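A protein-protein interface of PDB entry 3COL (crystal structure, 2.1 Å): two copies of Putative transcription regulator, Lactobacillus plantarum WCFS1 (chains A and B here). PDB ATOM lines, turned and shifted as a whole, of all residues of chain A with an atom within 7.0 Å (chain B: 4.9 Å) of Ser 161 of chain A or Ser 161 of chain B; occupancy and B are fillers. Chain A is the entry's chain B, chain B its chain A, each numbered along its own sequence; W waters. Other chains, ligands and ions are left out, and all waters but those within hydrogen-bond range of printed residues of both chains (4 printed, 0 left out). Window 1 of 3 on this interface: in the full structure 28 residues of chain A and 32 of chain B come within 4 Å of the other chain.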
ATOM      1  N   LEU A 107       0.332 -18.151   1.345  1.00  0.00           N
ATOM      2  CA  LEU A 107      -0.375 -17.185   0.447  1.00  0.00           C
ATOM      3  C   LEU A 107      -1.805 -17.582   0.230  1.00  0.00           C
ATOM      4  O   LEU A 107      -2.675 -16.716   0.108  1.00  0.00           O
ATOM      5  CB  LEU A 107       0.352 -16.942  -0.903  1.00  0.00           C
ATOM      6  CG  LEU A 107       1.201 -15.663  -1.020  1.00  0.00           C
ATOM      7  CD1 LEU A 107       2.114 -15.528   0.199  1.00  0.00           C
ATOM      8  CD2 LEU A 107       2.028 -15.651  -2.306  1.00  0.00           C
ATOM      9  N   GLN A 111      -3.972 -14.876   0.527  1.00  0.00           N
ATOM     10  CA  GLN A 111      -4.775 -14.651  -0.697  1.00  0.00           C
ATOM     11  C   GLN A 111      -6.244 -14.808  -0.415  1.00  0.00           C
ATOM     12  O   GLN A 111      -7.028 -13.996  -0.851  1.00  0.00           O
ATOM     13  CB  GLN A 111      -4.362 -15.556  -1.874  1.00  0.00           C
ATOM     14  CG  GLN A 111      -2.956 -15.254  -2.458  1.00  0.00           C
ATOM     15  CD  GLN A 111      -2.728 -13.782  -2.752  1.00  0.00           C
ATOM     16  OE1 GLN A 111      -3.068 -13.284  -3.827  1.00  0.00           O
ATOM     17  NE2 GLN A 111      -2.130 -13.083  -1.794  1.00  0.00           N
ATOM     18  N   LYS A 114      -7.627 -11.719   1.880  1.00  0.00           N
ATOM     19  CA  LYS A 114      -7.804 -10.571   0.970  1.00  0.00           C
ATOM     20  C   LYS A 114      -9.052 -10.746   0.105  1.00  0.00           C
ATOM     21  O   LYS A 114      -9.867  -9.804  -0.021  1.00  0.00           O
ATOM     22  CB  LYS A 114      -6.601 -10.396   0.038  1.00  0.00           C
ATOM     23  CG  LYS A 114      -5.471  -9.555   0.565  1.00  0.00           C
ATOM     24  CD  LYS A 114      -4.264  -9.703  -0.373  1.00  0.00           C
ATOM     25  CE  LYS A 114      -2.956  -9.606   0.401  1.00  0.00           C
ATOM     26  NZ  LYS A 114      -1.891 -10.404  -0.287  1.00  0.00           N
ATOM     27  N   LEU A 154      -3.267  -2.896  -7.254  1.00  0.00           N
ATOM     28  CA  LEU A 154      -3.028  -3.594  -8.521  1.00  0.00           C
ATOM     29  C   LEU A 154      -1.574  -4.057  -8.655  1.00  0.00           C
ATOM     30  O   LEU A 154      -1.332  -5.149  -9.146  1.00  0.00           O
ATOM     31  CB  LEU A 154      -3.440  -2.748  -9.734  1.00  0.00           C
ATOM     32  CG  LEU A 154      -4.931  -2.462  -9.969  1.00  0.00           C
ATOM     33  CD1 LEU A 154      -5.196  -2.091 -11.450  1.00  0.00           C
ATOM     34  CD2 LEU A 154      -5.815  -3.582  -9.574  1.00  0.00           C
ATOM     35  N   MET A 156       0.504  -4.599  -5.930  1.00  0.00           N
ATOM     36  CA  MET A 156       0.569  -5.664  -4.919  1.00  0.00           C
ATOM     37  C   MET A 156      -0.104  -6.920  -5.437  1.00  0.00           C
ATOM     38  O   MET A 156       0.418  -8.015  -5.270  1.00  0.00           O
ATOM     39  CB  MET A 156      -0.084  -5.223  -3.598  1.00  0.00           C
ATOM     40  CG  MET A 156       0.705  -4.159  -2.866  1.00  0.00           C
ATOM     41  SD  MET A 156       2.320  -4.931  -2.098  1.00  0.00           S
ATOM     42  CE  MET A 156       1.614  -5.315  -0.326  1.00  0.00           C
ATOM     43  N   GLY A 157      -1.263  -6.741  -6.070  1.00  0.00           N
ATOM     44  CA  GLY A 157      -2.061  -7.856  -6.634  1.00  0.00           C
ATOM     45  C   GLY A 157      -1.285  -8.731  -7.609  1.00  0.00           C
ATOM     46  O   GLY A 157      -1.268  -9.959  -7.489  1.00  0.00           O
ATOM     47  N   VAL A 158      -0.602  -8.115  -8.557  1.00  0.00           N
ATOM     48  CA  VAL A 158       0.071  -8.912  -9.564  1.00  0.00           C
ATOM     49  C   VAL A 158       1.261  -9.666  -8.963  1.00  0.00           C
ATOM     50  O   VAL A 158       1.544 -10.793  -9.379  1.00  0.00           O
ATOM     51  CB  VAL A 158       0.474  -8.104 -10.830  1.00  0.00           C
ATOM     52  CG1 VAL A 158       1.571  -7.065 -10.516  1.00  0.00           C
ATOM     53  CG2 VAL A 158       0.903  -9.061 -11.976  1.00  0.00           C
ATOM     54  N   VAL A 159       1.938  -9.055  -7.983  1.00  0.00           N
ATOM     55  CA  VAL A 159       3.023  -9.709  -7.269  1.00  0.00           C
ATOM     56  C   VAL A 159       2.497 -10.955  -6.545  1.00  0.00           C
ATOM     57  O   VAL A 159       3.039 -12.046  -6.697  1.00  0.00           O
ATOM     58  CB  VAL A 159       3.678  -8.761  -6.203  1.00  0.00           C
ATOM     59  CG1 VAL A 159       4.598  -9.565  -5.271  1.00  0.00           C
ATOM     60  CG2 VAL A 159       4.444  -7.569  -6.870  1.00  0.00           C
ATOM     61  N   PHE A 160       1.470 -10.773  -5.717  1.00  0.00           N
ATOM     62  CA  PHE A 160       0.961 -11.855  -4.884  1.00  0.00           C
ATOM     63  C   PHE A 160       0.220 -12.952  -5.670  1.00  0.00           C
ATOM     64  O   PHE A 160       0.442 -14.142  -5.400  1.00  0.00           O
ATOM     65  CB  PHE A 160       0.127 -11.314  -3.713  1.00  0.00           C
ATOM     66  CG  PHE A 160       0.976 -10.917  -2.522  1.00  0.00           C
ATOM     67  CD1 PHE A 160       1.185 -11.794  -1.466  1.00  0.00           C
ATOM     68  CD2 PHE A 160       1.626  -9.684  -2.497  1.00  0.00           C
ATOM     69  CE1 PHE A 160       1.988 -11.433  -0.380  1.00  0.00           C
ATOM     70  CE2 PHE A 160       2.436  -9.325  -1.430  1.00  0.00           C
ATOM     71  CZ  PHE A 160       2.623 -10.189  -0.363  1.00  0.00           C
ATOM     72  N   SER A 161      -0.634 -12.562  -6.630  1.00  0.00           N
ATOM     73  CA  SER A 161      -1.378 -13.570  -7.381  1.00  0.00           C
ATOM     74  C   SER A 161      -0.474 -14.371  -8.295  1.00  0.00           C
ATOM     75  O   SER A 161      -0.638 -15.583  -8.403  1.00  0.00           O
ATOM     76  CB  SER A 161      -2.562 -13.003  -8.180  1.00  0.00           C
ATOM     77  OG  SER A 161      -2.061 -12.068  -9.072  1.00  0.00           O
ATOM     78  N   THR A 162       0.498 -13.723  -8.934  1.00  0.00           N
ATOM     79  CA  THR A 162       1.420 -14.462  -9.818  1.00  0.00           C
ATOM     80  C   THR A 162       2.234 -15.498  -9.017  1.00  0.00           C
ATOM     81  O   THR A 162       2.326 -16.687  -9.389  1.00  0.00           O
ATOM     82  CB  THR A 162       2.369 -13.502 -10.551  1.00  0.00           C
ATOM     83  OG1 THR A 162       1.582 -12.619 -11.344  1.00  0.00           O
ATOM     84  CG2 THR A 162       3.300 -14.230 -11.500  1.00  0.00           C
ATOM     85  N   ILE A 163       2.818 -15.039  -7.916  1.00  0.00           N
ATOM     86  CA  ILE A 163       3.576 -15.922  -7.047  1.00  0.00           C
ATOM     87  C   ILE A 163       2.676 -17.012  -6.480  1.00  0.00           C
ATOM     88  O   ILE A 163       3.098 -18.135  -6.422  1.00  0.00           O
ATOM     89  CB  ILE A 163       4.356 -15.161  -5.936  1.00  0.00           C
ATOM     90  CG1 ILE A 163       5.530 -14.371  -6.573  1.00  0.00           C
ATOM     91  CG2 ILE A 163       4.969 -16.163  -4.943  1.00  0.00           C
ATOM     92  CD1 ILE A 163       6.057 -13.261  -5.667  1.00  0.00           C
ATOM     93  N   HIS A 164       1.440 -16.690  -6.107  1.00  0.00           N
ATOM     94  CA  HIS A 164       0.520 -17.687  -5.559  1.00  0.00           C
ATOM     95  C   HIS A 164       0.148 -18.773  -6.558  1.00  0.00           C
ATOM     96  O   HIS A 164       0.158 -19.936  -6.235  1.00  0.00           O
ATOM     97  CB  HIS A 164      -0.778 -17.034  -5.050  1.00  0.00           C
ATOM     98  CG  HIS A 164      -1.711 -18.000  -4.379  1.00  0.00           C
ATOM     99  ND1 HIS A 164      -3.077 -17.928  -4.518  1.00  0.00           N
ATOM    100  CD2 HIS A 164      -1.476 -19.039  -3.549  1.00  0.00           C
ATOM    101  CE1 HIS A 164      -3.647 -18.889  -3.808  1.00  0.00           C
ATOM    102  NE2 HIS A 164      -2.695 -19.586  -3.221  1.00  0.00           N
ATOM    103  N   THR A 165      -0.221 -18.382  -7.768  1.00  0.00           N
ATOM    104  CA  THR A 165      -0.503 -19.352  -8.816  1.00  0.00           C
ATOM    105  C   THR A 165       0.673 -20.282  -9.081  1.00  0.00           C
ATOM    106  O   THR A 165       0.483 -21.454  -9.281  1.00  0.00           O
ATOM    107  CB  THR A 165      -0.856 -18.614 -10.124  1.00  0.00           C
ATOM    108  OG1 THR A 165      -1.905 -17.697  -9.835  1.00  0.00           O
ATOM    109  CG2 THR A 165      -1.354 -19.607 -11.189  1.00  0.00           C
ATOM    110  N   HIS A 166       1.891 -19.749  -9.080  1.00  0.00           N
ATOM    111  CA  HIS A 166       3.094 -20.525  -9.381  1.00  0.00           C
ATOM    112  C   HIS A 166       3.367 -21.534  -8.253  1.00  0.00           C
ATOM    113  O   HIS A 166       3.579 -22.719  -8.507  1.00  0.00           O
ATOM    114  CB  HIS A 166       4.245 -19.553  -9.556  1.00  0.00           C
ATOM    115  CG  HIS A 166       5.584 -20.191  -9.764  1.00  0.00           C
ATOM    116  ND1 HIS A 166       5.853 -21.042 -10.809  1.00  0.00           N
ATOM    117  CD2 HIS A 166       6.755 -20.032  -9.100  1.00  0.00           C
ATOM    118  CE1 HIS A 166       7.129 -21.392 -10.774  1.00  0.00           C
ATOM    119  NE2 HIS A 166       7.696 -20.801  -9.743  1.00  0.00           N
ATOM    120  N   THR A 167       3.271 -21.055  -7.013  1.00  0.00           N
ATOM    121  CA  THR A 167       3.381 -21.876  -5.803  1.00  0.00           C
ATOM    122  C   THR A 167       2.350 -22.994  -5.803  1.00  0.00           C
ATOM    123  O   THR A 167       2.679 -24.159  -5.520  1.00  0.00           O
ATOM    124  CB  THR A 167       3.108 -21.006  -4.577  1.00  0.00           C
ATOM    125  OG1 THR A 167       4.103 -19.974  -4.523  1.00  0.00           O
ATOM    126  CG2 THR A 167       3.153 -21.821  -3.293  1.00  0.00           C
ATOM    127  N   ILE A 189       6.118 -10.214 -13.657  1.00  0.00           N
ATOM    128  CA  ILE A 189       5.696  -9.345 -12.576  1.00  0.00           C
ATOM    129  C   ILE A 189       6.228  -7.936 -12.777  1.00  0.00           C
ATOM    130  O   ILE A 189       5.467  -6.972 -12.694  1.00  0.00           O
ATOM    131  CB  ILE A 189       6.109  -9.907 -11.177  1.00  0.00           C
ATOM    132  CG1 ILE A 189       5.278 -11.190 -10.887  1.00  0.00           C
ATOM    133  CG2 ILE A 189       5.894  -8.812 -10.083  1.00  0.00           C
ATOM    134  CD1 ILE A 189       5.766 -12.028  -9.658  1.00  0.00           C
ATOM    135  N   MET B 156      -3.546 -16.630 -17.653  1.00  0.00           N
ATOM    136  CA  MET B 156      -4.927 -16.600 -17.130  1.00  0.00           C
ATOM    137  C   MET B 156      -5.007 -15.851 -15.804  1.00  0.00           C
ATOM    138  O   MET B 156      -5.868 -15.001 -15.600  1.00  0.00           O
ATOM    139  CB  MET B 156      -5.442 -18.029 -16.921  1.00  0.00           C
ATOM    140  CG  MET B 156      -5.785 -18.757 -18.214  1.00  0.00           C
ATOM    141  SD  MET B 156      -7.152 -17.766 -19.190  1.00  0.00           S
ATOM    142  CE  MET B 156      -8.714 -18.181 -18.074  1.00  0.00           C
ATOM    143  N   GLY B 157      -4.086 -16.185 -14.912  1.00  0.00           N
ATOM    144  CA  GLY B 157      -4.016 -15.625 -13.545  1.00  0.00           C
ATOM    145  C   GLY B 157      -3.859 -14.114 -13.519  1.00  0.00           C
ATOM    146  O   GLY B 157      -4.572 -13.428 -12.769  1.00  0.00           O
ATOM    147  N   VAL B 158      -2.948 -13.577 -14.330  1.00  0.00           N
ATOM    148  CA  VAL B 158      -2.750 -12.135 -14.391  1.00  0.00           C
ATOM    149  C   VAL B 158      -3.986 -11.380 -14.936  1.00  0.00           C
ATOM    150  O   VAL B 158      -4.348 -10.313 -14.406  1.00  0.00           O
ATOM    151  CB  VAL B 158      -1.422 -11.727 -15.134  1.00  0.00           C
ATOM    152  CG1 VAL B 158      -1.462 -12.060 -16.641  1.00  0.00           C
ATOM    153  CG2 VAL B 158      -1.201 -10.237 -14.983  1.00  0.00           C
ATOM    154  N   VAL B 159      -4.624 -11.941 -15.974  1.00  0.00           N
ATOM    155  CA  VAL B 159      -5.864 -11.432 -16.516  1.00  0.00           C
ATOM    156  C   VAL B 159      -6.944 -11.390 -15.442  1.00  0.00           C
ATOM    157  O   VAL B 159      -7.560 -10.349 -15.187  1.00  0.00           O
ATOM    158  CB  VAL B 159      -6.347 -12.312 -17.700  1.00  0.00           C
ATOM    159  CG1 VAL B 159      -7.813 -11.887 -18.191  1.00  0.00           C
ATOM    160  CG2 VAL B 159      -5.381 -12.204 -18.835  1.00  0.00           C
ATOM    161  N   PHE B 160      -7.215 -12.522 -14.832  1.00  0.00           N
ATOM    162  CA  PHE B 160      -8.322 -12.585 -13.905  1.00  0.00           C
ATOM    163  C   PHE B 160      -8.077 -11.872 -12.602  1.00  0.00           C
ATOM    164  O   PHE B 160      -8.984 -11.191 -12.079  1.00  0.00           O
ATOM    165  CB  PHE B 160      -8.786 -14.044 -13.711  1.00  0.00           C
ATOM    166  CG  PHE B 160      -9.674 -14.495 -14.827  1.00  0.00           C
ATOM    167  CD1 PHE B 160     -11.047 -14.513 -14.669  1.00  0.00           C
ATOM    168  CD2 PHE B 160      -9.130 -14.819 -16.084  1.00  0.00           C
ATOM    169  CE1 PHE B 160     -11.863 -14.895 -15.723  1.00  0.00           C
ATOM    170  CE2 PHE B 160      -9.928 -15.183 -17.124  1.00  0.00           C
ATOM    171  CZ  PHE B 160     -11.300 -15.215 -16.960  1.00  0.00           C
ATOM    172  N   SER B 161      -6.863 -12.014 -12.064  1.00  0.00           N
ATOM    173  CA  SER B 161      -6.543 -11.393 -10.760  1.00  0.00           C
ATOM    174  C   SER B 161      -6.553  -9.870 -10.805  1.00  0.00           C
ATOM    175  O   SER B 161      -7.104  -9.230  -9.914  1.00  0.00           O
ATOM    176  CB  SER B 161      -5.222 -11.908 -10.209  1.00  0.00           C
ATOM    177  OG  SER B 161      -4.821 -11.147  -9.090  1.00  0.00           O
ATOM    178  N   THR B 162      -5.979  -9.307 -11.862  1.00  0.00           N
ATOM    179  CA  THR B 162      -5.937  -7.840 -12.084  1.00  0.00           C
ATOM    180  C   THR B 162      -7.354  -7.264 -12.270  1.00  0.00           C
ATOM    181  O   THR B 162      -7.681  -6.265 -11.658  1.00  0.00           O
ATOM    182  CB  THR B 162      -5.070  -7.463 -13.313  1.00  0.00           C
ATOM    183  OG1 THR B 162      -3.740  -7.968 -13.107  1.00  0.00           O
ATOM    184  CG2 THR B 162      -4.995  -5.933 -13.551  1.00  0.00           C
ATOM    185  N   ILE B 163      -8.165  -7.910 -13.116  1.00  0.00           N
ATOM    186  CA  ILE B 163      -9.539  -7.490 -13.301  1.00  0.00           C
ATOM    187  C   ILE B 163     -10.353  -7.673 -12.028  1.00  0.00           C
ATOM    188  O   ILE B 163     -11.174  -6.829 -11.681  1.00  0.00           O
ATOM    189  CB  ILE B 163     -10.174  -8.199 -14.525  1.00  0.00           C
ATOM    190  CG1 ILE B 163      -9.518  -7.657 -15.814  1.00  0.00           C
ATOM    191  CG2 ILE B 163     -11.694  -8.050 -14.513  1.00  0.00           C
ATOM    192  CD1 ILE B 163      -9.824  -8.498 -17.100  1.00  0.00           C
ATOM    193  N   HIS B 164     -10.131  -8.774 -11.315  1.00  0.00           N
ATOM    194  CA  HIS B 164     -10.886  -8.983 -10.105  1.00  0.00           C
ATOM    195  C   HIS B 164     -10.592  -7.898  -9.054  1.00  0.00           C
ATOM    196  O   HIS B 164     -11.515  -7.344  -8.500  1.00  0.00           O
ATOM    197  CB  HIS B 164     -10.647 -10.387  -9.545  1.00  0.00           C
ATOM    198  CG  HIS B 164     -11.549 -10.726  -8.413  1.00  0.00           C
ATOM    199  ND1 HIS B 164     -11.199 -11.611  -7.424  1.00  0.00           N
ATOM    200  CD2 HIS B 164     -12.791 -10.291  -8.103  1.00  0.00           C
ATOM    201  CE1 HIS B 164     -12.184 -11.700  -6.545  1.00  0.00           C
ATOM    202  NE2 HIS B 164     -13.157 -10.908  -6.934  1.00  0.00           N
ATOM    203  N   THR B 165      -9.312  -7.611  -8.801  1.00  0.00           N
ATOM    204  CA  THR B 165      -8.885  -6.577  -7.849  1.00  0.00           C
ATOM    205  C   THR B 165      -9.471  -5.208  -8.217  1.00  0.00           C
ATOM    206  O   THR B 165      -9.995  -4.491  -7.367  1.00  0.00           O
ATOM    207  CB  THR B 165      -7.348  -6.491  -7.747  1.00  0.00           C
ATOM    208  OG1 THR B 165      -6.805  -7.776  -7.386  1.00  0.00           O
ATOM    209  CG2 THR B 165      -6.914  -5.490  -6.680  1.00  0.00           C
HETATM  210  O   HOH W   1      -2.976  -9.493 -10.828  1.00  0.00           O
HETATM  211  O   HOH W   2      -0.181 -14.850 -12.878  1.00  0.00           O
HETATM  212  O   HOH W   3      -1.239 -12.874 -11.430  1.00  0.00           O
HETATM  213  O   HOH W   4      -3.246  -6.630 -10.411  1.00  0.00           O
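OG of Ser 161 of chain B lies within hydrogen-bond range of OG of Ser 161 of chain A (2.9 Å).
The backbone carbonyl oxygen of Val 158 of chain B lies within hydrogen-bond range of the side-chain hydroxyl of Thr 162 of chain B (2.7 Å).
OG1 of Thr 165 of chain B is in hydrogen-bond range of O of Ser 161 of chain B (2.9 Å).
The backbone carbonyl oxygen of Gly 157 of chain A is in hydrogen-bond range of the side-chain hydroxyl of Ser 161 of chain A (2.8 Å).
OG1 of Thr 162 of chain A sits at hydrogen-bond distance from O of Val 158 of chain A, at 2.7 Å.
O of Ser 161 of chain A lies within hydrogen-bond range of OG1 of Thr 165 of chain A (2.9 Å).
Among the printed residues, pairs that only touch across the chains: Leu 154 of chain A with Thr 162 of chain B, Leu 154 of chain A with Thr 165 of chain B and Val 158 of chain A with Val 158 of chain B.
Printed residues of chain B within 4 Å of Leu 154 of chain A: Thr 162 and Thr 165.
Printed residues of chain B within 4 Å of Val 158 of chain A: Val 158.
Printed residues of chain B within 4 Å of Ser 161 of chain A: Ser 161 (2.9 Å).
Thr 162 of chain A touches none of the printed residues of chain B.
Printed residues of chain A within 4 Å of Ser 161 of chain B: Ser 161 (2.9 Å).
Printed residues of chain A within 4 Å of Thr 162 of chain B: Leu 154.
His 164 of chain B touches none of the printed residues of chain A.
Printed residues of chain A within 4 Å of Thr 165 of chain B: Leu 154.
The nearest printed residue of chain A that does not touch Ser 161 of chain B is Gly 157 of chain A (4.1 Å).
The nearest printed residue of chain A that does not touch Thr 165 of chain B is Gly 157 of chain A (4.8 Å).
Hydrophobic or aromatic side chains of chain B that line the printed part of chain A: Val 158.
Of the 17 printed residues of chain A, 3 touch a printed residue of chain B.
Along chain A the printed residues that touch a printed residue of chain B span positions 154 to 161.
Among the printed residues, no Asp or Glu carboxylate lies within 4 Å of a Lys or Arg side-chain nitrogen of the other chain.
Val 158 of chain A touches its own counterpart, Val 158 of chain B.
Ser 161 of chain B touches its own counterpart, Ser 161 of chain A.
Water W3 lies within hydrogen-bond range of the side-chain hydroxyl of Ser 161 of chain A, the side-chain hydroxyl of Thr 162 of chain A and the backbone NH of Val 158 of chain B.
Water W4 lies within hydrogen-bond range of the backbone carbonyl oxygen of Leu 154 of chain A and the side-chain hydroxyl of Thr 162 of chain B.
Water W1 lies within hydrogen-bond range of OG1 of Thr 162 of chain B (2.8 Å), OG of Ser 161 of chain B (3.0 Å) and OG of Ser 161 of chain A (3.2 Å).
Water W2 bridges the side-chain hydroxyl (OG1) of Thr 162 of chain A (3.2 Å) and the backbone NH (N) of Val 158 of chain B (3.4 Å).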
